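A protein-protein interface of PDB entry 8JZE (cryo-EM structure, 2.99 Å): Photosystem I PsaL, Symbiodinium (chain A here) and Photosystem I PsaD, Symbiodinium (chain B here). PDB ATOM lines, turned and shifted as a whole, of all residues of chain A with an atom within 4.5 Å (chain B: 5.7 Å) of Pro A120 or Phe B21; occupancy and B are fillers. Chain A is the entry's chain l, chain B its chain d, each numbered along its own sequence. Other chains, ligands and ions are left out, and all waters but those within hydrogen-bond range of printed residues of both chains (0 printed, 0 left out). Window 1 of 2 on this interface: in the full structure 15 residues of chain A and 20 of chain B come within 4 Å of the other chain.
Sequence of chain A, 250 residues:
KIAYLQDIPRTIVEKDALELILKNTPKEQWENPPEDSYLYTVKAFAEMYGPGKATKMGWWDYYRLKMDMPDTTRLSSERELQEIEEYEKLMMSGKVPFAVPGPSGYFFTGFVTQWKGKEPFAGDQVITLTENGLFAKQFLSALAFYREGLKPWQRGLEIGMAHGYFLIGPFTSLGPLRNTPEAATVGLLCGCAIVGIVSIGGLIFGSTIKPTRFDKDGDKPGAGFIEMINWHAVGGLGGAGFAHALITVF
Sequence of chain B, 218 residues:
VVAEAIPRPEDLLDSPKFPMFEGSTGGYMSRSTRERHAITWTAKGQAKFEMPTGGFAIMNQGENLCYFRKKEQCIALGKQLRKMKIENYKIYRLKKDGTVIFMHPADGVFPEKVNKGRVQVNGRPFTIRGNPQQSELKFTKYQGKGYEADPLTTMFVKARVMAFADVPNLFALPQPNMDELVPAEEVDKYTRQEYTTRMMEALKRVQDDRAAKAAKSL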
ATOM      1  N   MET A  92      -0.560 -22.543  -2.271  1.00  0.00           N
ATOM      2  CA  MET A  92       0.141 -23.652  -1.639  1.00  0.00           C
ATOM      3  C   MET A  92      -0.199 -24.994  -2.271  1.00  0.00           C
ATOM      4  O   MET A  92       0.612 -25.922  -2.192  1.00  0.00           O
ATOM      5  CB  MET A  92      -0.172 -23.692  -0.141  1.00  0.00           C
ATOM      6  CG  MET A  92       0.811 -24.513   0.678  1.00  0.00           C
ATOM      7  SD  MET A  92       2.484 -23.847   0.630  1.00  0.00           S
ATOM      8  CE  MET A  92       2.265 -22.309   1.516  1.00  0.00           C
ATOM      9  N   LYS A 116       2.637 -26.417 -10.748  1.00  0.00           N
ATOM     10  CA  LYS A 116       3.683 -27.420 -10.591  1.00  0.00           C
ATOM     11  C   LYS A 116       3.500 -28.542 -11.604  1.00  0.00           C
ATOM     12  O   LYS A 116       2.394 -29.047 -11.805  1.00  0.00           O
ATOM     13  CB  LYS A 116       3.675 -27.991  -9.173  1.00  0.00           C
ATOM     14  CG  LYS A 116       4.104 -27.007  -8.099  1.00  0.00           C
ATOM     15  CD  LYS A 116       4.322 -27.703  -6.765  1.00  0.00           C
ATOM     16  CE  LYS A 116       3.074 -28.444  -6.314  1.00  0.00           C
ATOM     17  NZ  LYS A 116       3.270 -29.125  -5.004  1.00  0.00           N
ATOM     18  N   GLY A 117       4.598 -28.942 -12.235  1.00  0.00           N
ATOM     19  CA  GLY A 117       4.560 -29.971 -13.250  1.00  0.00           C
ATOM     20  C   GLY A 117       4.433 -31.361 -12.658  1.00  0.00           C
ATOM     21  O   GLY A 117       4.126 -31.552 -11.481  1.00  0.00           O
ATOM     22  N   LYS A 118       4.668 -32.356 -13.517  1.00  0.00           N
ATOM     23  CA  LYS A 118       4.612 -33.742 -13.067  1.00  0.00           C
ATOM     24  C   LYS A 118       5.697 -34.029 -12.038  1.00  0.00           C
ATOM     25  O   LYS A 118       5.465 -34.764 -11.071  1.00  0.00           O
ATOM     26  CB  LYS A 118       4.721 -34.686 -14.264  1.00  0.00           C
ATOM     27  CG  LYS A 118       3.456 -34.738 -15.109  1.00  0.00           C
ATOM     28  CD  LYS A 118       3.658 -35.541 -16.382  1.00  0.00           C
ATOM     29  CE  LYS A 118       4.635 -34.851 -17.316  1.00  0.00           C
ATOM     30  NZ  LYS A 118       4.786 -35.594 -18.597  1.00  0.00           N
ATOM     31  N   GLU A 119       6.889 -33.467 -12.231  1.00  0.00           N
ATOM     32  CA  GLU A 119       7.912 -33.482 -11.195  1.00  0.00           C
ATOM     33  C   GLU A 119       7.809 -32.182 -10.409  1.00  0.00           C
ATOM     34  O   GLU A 119       8.335 -31.150 -10.844  1.00  0.00           O
ATOM     35  CB  GLU A 119       9.312 -33.641 -11.790  1.00  0.00           C
ATOM     36  CG  GLU A 119       9.516 -34.900 -12.614  1.00  0.00           C
ATOM     37  CD  GLU A 119      10.969 -35.115 -12.996  1.00  0.00           C
ATOM     38  OE1 GLU A 119      11.853 -34.545 -12.323  1.00  0.00           O
ATOM     39  OE2 GLU A 119      11.228 -35.850 -13.971  1.00  0.00           O
ATOM     40  N   PRO A 120       7.137 -32.190  -9.253  1.00  0.00           N
ATOM     41  CA  PRO A 120       6.871 -30.924  -8.554  1.00  0.00           C
ATOM     42  C   PRO A 120       8.122 -30.176  -8.137  1.00  0.00           C
ATOM     43  O   PRO A 120       8.086 -28.943  -8.029  1.00  0.00           O
ATOM     44  CB  PRO A 120       6.041 -31.366  -7.341  1.00  0.00           C
ATOM     45  CG  PRO A 120       6.393 -32.793  -7.137  1.00  0.00           C
ATOM     46  CD  PRO A 120       6.629 -33.351  -8.506  1.00  0.00           C
ATOM     47  N   PHE A 121       9.230 -30.874  -7.898  1.00  0.00           N
ATOM     48  CA  PHE A 121      10.475 -30.223  -7.516  1.00  0.00           C
ATOM     49  C   PHE A 121      11.310 -29.778  -8.710  1.00  0.00           C
ATOM     50  O   PHE A 121      12.323 -29.099  -8.513  1.00  0.00           O
ATOM     51  CB  PHE A 121      11.310 -31.152  -6.631  1.00  0.00           C
ATOM     52  CG  PHE A 121      10.655 -31.502  -5.327  1.00  0.00           C
ATOM     53  CD1 PHE A 121      10.683 -30.616  -4.263  1.00  0.00           C
ATOM     54  CD2 PHE A 121      10.022 -32.722  -5.162  1.00  0.00           C
ATOM     55  CE1 PHE A 121      10.085 -30.936  -3.061  1.00  0.00           C
ATOM     56  CE2 PHE A 121       9.422 -33.049  -3.963  1.00  0.00           C
ATOM     57  CZ  PHE A 121       9.453 -32.155  -2.910  1.00  0.00           C
ATOM     58  N   ALA A 122      10.920 -30.137  -9.932  1.00  0.00           N
ATOM     59  CA  ALA A 122      11.663 -29.730 -11.117  1.00  0.00           C
ATOM     60  C   ALA A 122      11.341 -28.282 -11.464  1.00  0.00           C
ATOM     61  O   ALA A 122      10.173 -27.881 -11.474  1.00  0.00           O
ATOM     62  CB  ALA A 122      11.334 -30.641 -12.298  1.00  0.00           C
ATOM     63  N   LEU B  13       6.557 -39.517  -9.005  1.00  0.00           N
ATOM     64  CA  LEU B  13       5.547 -38.481  -9.160  1.00  0.00           C
ATOM     65  C   LEU B  13       4.393 -38.731  -8.195  1.00  0.00           C
ATOM     66  O   LEU B  13       3.961 -39.872  -8.005  1.00  0.00           O
ATOM     67  CB  LEU B  13       5.035 -38.454 -10.602  1.00  0.00           C
ATOM     68  CG  LEU B  13       6.064 -38.630 -11.721  1.00  0.00           C
ATOM     69  CD1 LEU B  13       5.381 -38.683 -13.077  1.00  0.00           C
ATOM     70  CD2 LEU B  13       7.097 -37.520 -11.688  1.00  0.00           C
ATOM     71  N   ASP B  14       3.899 -37.655  -7.579  1.00  0.00           N
ATOM     72  CA  ASP B  14       2.732 -37.692  -6.697  1.00  0.00           C
ATOM     73  C   ASP B  14       2.954 -38.651  -5.522  1.00  0.00           C
ATOM     74  O   ASP B  14       2.302 -39.687  -5.383  1.00  0.00           O
ATOM     75  CB  ASP B  14       1.469 -38.062  -7.484  1.00  0.00           C
ATOM     76  CG  ASP B  14       1.185 -37.097  -8.616  1.00  0.00           C
ATOM     77  OD1 ASP B  14       1.434 -35.886  -8.443  1.00  0.00           O
ATOM     78  OD2 ASP B  14       0.718 -37.551  -9.683  1.00  0.00           O
ATOM     79  N   PHE B  18       5.718 -35.825  -0.102  1.00  0.00           N
ATOM     80  CA  PHE B  18       6.071 -34.485  -0.552  1.00  0.00           C
ATOM     81  C   PHE B  18       5.316 -33.443   0.265  1.00  0.00           C
ATOM     82  O   PHE B  18       4.085 -33.513   0.365  1.00  0.00           O
ATOM     83  CB  PHE B  18       5.760 -34.319  -2.038  1.00  0.00           C
ATOM     84  CG  PHE B  18       6.634 -35.144  -2.940  1.00  0.00           C
ATOM     85  CD1 PHE B  18       7.832 -35.667  -2.479  1.00  0.00           C
ATOM     86  CD2 PHE B  18       6.259 -35.394  -4.249  1.00  0.00           C
ATOM     87  CE1 PHE B  18       8.638 -36.425  -3.307  1.00  0.00           C
ATOM     88  CE2 PHE B  18       7.060 -36.150  -5.083  1.00  0.00           C
ATOM     89  CZ  PHE B  18       8.251 -36.667  -4.611  1.00  0.00           C
ATOM     90  N   PRO B  19       6.006 -32.479   0.870  1.00  0.00           N
ATOM     91  CA  PRO B  19       5.303 -31.392   1.553  1.00  0.00           C
ATOM     92  C   PRO B  19       4.567 -30.514   0.555  1.00  0.00           C
ATOM     93  O   PRO B  19       4.930 -30.428  -0.619  1.00  0.00           O
ATOM     94  CB  PRO B  19       6.432 -30.621   2.244  1.00  0.00           C
ATOM     95  CG  PRO B  19       7.625 -30.885   1.397  1.00  0.00           C
ATOM     96  CD  PRO B  19       7.468 -32.302   0.915  1.00  0.00           C
ATOM     97  N   MET B  20       3.512 -29.864   1.034  1.00  0.00           N
ATOM     98  CA  MET B  20       2.782 -28.905   0.209  1.00  0.00           C
ATOM     99  C   MET B  20       3.658 -27.677   0.010  1.00  0.00           C
ATOM    100  O   MET B  20       3.832 -26.869   0.923  1.00  0.00           O
ATOM    101  CB  MET B  20       1.455 -28.528   0.858  1.00  0.00           C
ATOM    102  CG  MET B  20       0.399 -29.617   0.830  1.00  0.00           C
ATOM    103  SD  MET B  20      -1.170 -29.043   1.508  1.00  0.00           S
ATOM    104  CE  MET B  20      -0.656 -28.507   3.136  1.00  0.00           C
ATOM    105  N   PHE B  21       4.218 -27.531  -1.189  1.00  0.00           N
ATOM    106  CA  PHE B  21       5.046 -26.384  -1.525  1.00  0.00           C
ATOM    107  C   PHE B  21       4.532 -25.741  -2.804  1.00  0.00           C
ATOM    108  O   PHE B  21       3.972 -26.411  -3.676  1.00  0.00           O
ATOM    109  CB  PHE B  21       6.529 -26.765  -1.675  1.00  0.00           C
ATOM    110  CG  PHE B  21       6.826 -27.639  -2.856  1.00  0.00           C
ATOM    111  CD1 PHE B  21       6.498 -28.982  -2.841  1.00  0.00           C
ATOM    112  CD2 PHE B  21       7.471 -27.121  -3.966  1.00  0.00           C
ATOM    113  CE1 PHE B  21       6.782 -29.788  -3.918  1.00  0.00           C
ATOM    114  CE2 PHE B  21       7.759 -27.922  -5.046  1.00  0.00           C
ATOM    115  CZ  PHE B  21       7.416 -29.257  -5.021  1.00  0.00           C
ATOM    116  N   GLU B  22       4.730 -24.425  -2.899  1.00  0.00           N
ATOM    117  CA  GLU B  22       4.131 -23.655  -3.984  1.00  0.00           C
ATOM    118  C   GLU B  22       4.677 -24.076  -5.342  1.00  0.00           C
ATOM    119  O   GLU B  22       3.921 -24.189  -6.313  1.00  0.00           O
ATOM    120  CB  GLU B  22       4.358 -22.163  -3.740  1.00  0.00           C
ATOM    121  CG  GLU B  22       3.817 -21.686  -2.399  1.00  0.00           C
ATOM    122  CD  GLU B  22       4.159 -20.240  -2.096  1.00  0.00           C
ATOM    123  OE1 GLU B  22       5.072 -19.689  -2.744  1.00  0.00           O
ATOM    124  OE2 GLU B  22       3.510 -19.655  -1.203  1.00  0.00           O
ATOM    125  N   GLY B  23       5.982 -24.310  -5.434  1.00  0.00           N
ATOM    126  CA  GLY B  23       6.580 -24.697  -6.695  1.00  0.00           C
ATOM    127  C   GLY B  23       6.979 -23.495  -7.523  1.00  0.00           C
ATOM    128  O   GLY B  23       6.146 -22.636  -7.817  1.00  0.00           O
ATOM    129  N   SER B  24       8.251 -23.422  -7.906  1.00  0.00           N
ATOM    130  CA  SER B  24       8.777 -22.270  -8.621  1.00  0.00           C
ATOM    131  C   SER B  24       9.717 -22.751  -9.718  1.00  0.00           C
ATOM    132  O   SER B  24       9.927 -23.953  -9.906  1.00  0.00           O
ATOM    133  CB  SER B  24       9.493 -21.311  -7.663  1.00  0.00           C
ATOM    134  OG  SER B  24      10.615 -21.933  -7.063  1.00  0.00           O
ATOM    135  N   MET B  51      11.354 -23.060   1.082  1.00  0.00           N
ATOM    136  CA  MET B  51      12.157 -23.913   0.221  1.00  0.00           C
ATOM    137  C   MET B  51      13.442 -23.193  -0.175  1.00  0.00           C
ATOM    138  O   MET B  51      13.437 -21.973  -0.371  1.00  0.00           O
ATOM    139  CB  MET B  51      11.374 -24.301  -1.031  1.00  0.00           C
ATOM    140  CG  MET B  51      10.110 -25.092  -0.760  1.00  0.00           C
ATOM    141  SD  MET B  51      10.442 -26.808  -0.333  1.00  0.00           S
ATOM    142  CE  MET B  51      11.230 -27.366  -1.838  1.00  0.00           C
ATOM    143  N   PHE B  56       7.448 -20.962  -0.513  1.00  0.00           N
ATOM    144  CA  PHE B  56       7.293 -21.522   0.820  1.00  0.00           C
ATOM    145  C   PHE B  56       6.643 -22.899   0.748  1.00  0.00           C
ATOM    146  O   PHE B  56       6.143 -23.329  -0.293  1.00  0.00           O
ATOM    147  CB  PHE B  56       6.477 -20.577   1.706  1.00  0.00           C
ATOM    148  CG  PHE B  56       7.188 -19.295   2.030  1.00  0.00           C
ATOM    149  CD1 PHE B  56       7.104 -18.206   1.179  1.00  0.00           C
ATOM    150  CD2 PHE B  56       7.945 -19.182   3.184  1.00  0.00           C
ATOM    151  CE1 PHE B  56       7.759 -17.027   1.475  1.00  0.00           C
ATOM    152  CE2 PHE B  56       8.602 -18.007   3.486  1.00  0.00           C
ATOM    153  CZ  PHE B  56       8.509 -16.927   2.630  1.00  0.00           C
ATOM    154  N   ALA B  57       6.666 -23.597   1.880  1.00  0.00           N
ATOM    155  CA  ALA B  57       6.181 -24.965   1.939  1.00  0.00           C
ATOM    156  C   ALA B  57       5.632 -25.250   3.327  1.00  0.00           C
ATOM    157  O   ALA B  57       5.973 -24.579   4.302  1.00  0.00           O
ATOM    158  CB  ALA B  57       7.287 -25.967   1.597  1.00  0.00           C
ATOM    159  N   ILE B  58       4.778 -26.266   3.402  1.00  0.00           N
ATOM    160  CA  ILE B  58       4.207 -26.735   4.658  1.00  0.00           C
ATOM    161  C   ILE B  58       4.563 -28.207   4.801  1.00  0.00           C
ATOM    162  O   ILE B  58       4.251 -29.013   3.916  1.00  0.00           O
ATOM    163  CB  ILE B  58       2.687 -26.527   4.712  1.00  0.00           C
ATOM    164  CG1 ILE B  58       2.348 -25.038   4.594  1.00  0.00           C
ATOM    165  CG2 ILE B  58       2.114 -27.106   5.993  1.00  0.00           C
ATOM    166  CD1 ILE B  58       0.867 -24.743   4.643  1.00  0.00           C
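The backbone carbonyl oxygen (O) of Phe B56 lies within hydrogen-bond range of the backbone NH (N) of Glu B22 (3.2 Å). The backbone carbonyl oxygen (O) of Met B20 lies within hydrogen-bond range of the backbone NH (N) of Ile B58, 2.7 Å away.
Among the printed residues, pairs that only touch across the chains: Pro A120 with Phe B21, Lys A118 with Leu B13, Lys A116 with Glu B22, Phe A121 with Phe B18, Phe A121 with Phe B21, Lys A116 with Gly B23, Glu A119 with Leu B13, Met A92 with Phe B21, Met A92 with Phe B56, Pro A120 with Phe B18, Phe A121 with Met B51, Met A92 with Glu B22 and Met A92 with Ile B58.
Of the printed residues of chain A, Phe B21 touches Met A92, Lys A116, Pro A120 and Phe A121. Of the printed residues of chain B, Met A92 touches Met B20 (3.3 Å), Phe B21 (3.7 Å), Glu B22 (3.95 Å), Phe B56 (3.8 Å) and Ile B58 (3.97 Å). Of the printed residues of chain A, Leu B13 touches Lys A118 and Glu A119. Of the printed residues of chain B, Glu A119 touches Leu B13 (3.7 Å). Printed residues of chain A within 4 Å of Met B20: Met A92. The nearest printed residue of chain A that does not touch Phe B21 is Ala A122 (6.1 Å).
The side-chain amino group of Lys A116 sits at hydrogen-bond distance from the backbone carbonyl oxygen of Phe B21 (3.1 Å). O of Met B20 lies close to SD of Met A92 (3.3 Å).
Of the 13 printed residues of chain B, 9 touch a printed residue of chain A. Among the printed residues, 15 pairs touch across the chains. Among the printed residues, no Asp or Glu carboxylate lies within 4 Å of a Lys or Arg side-chain nitrogen of the other chain.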
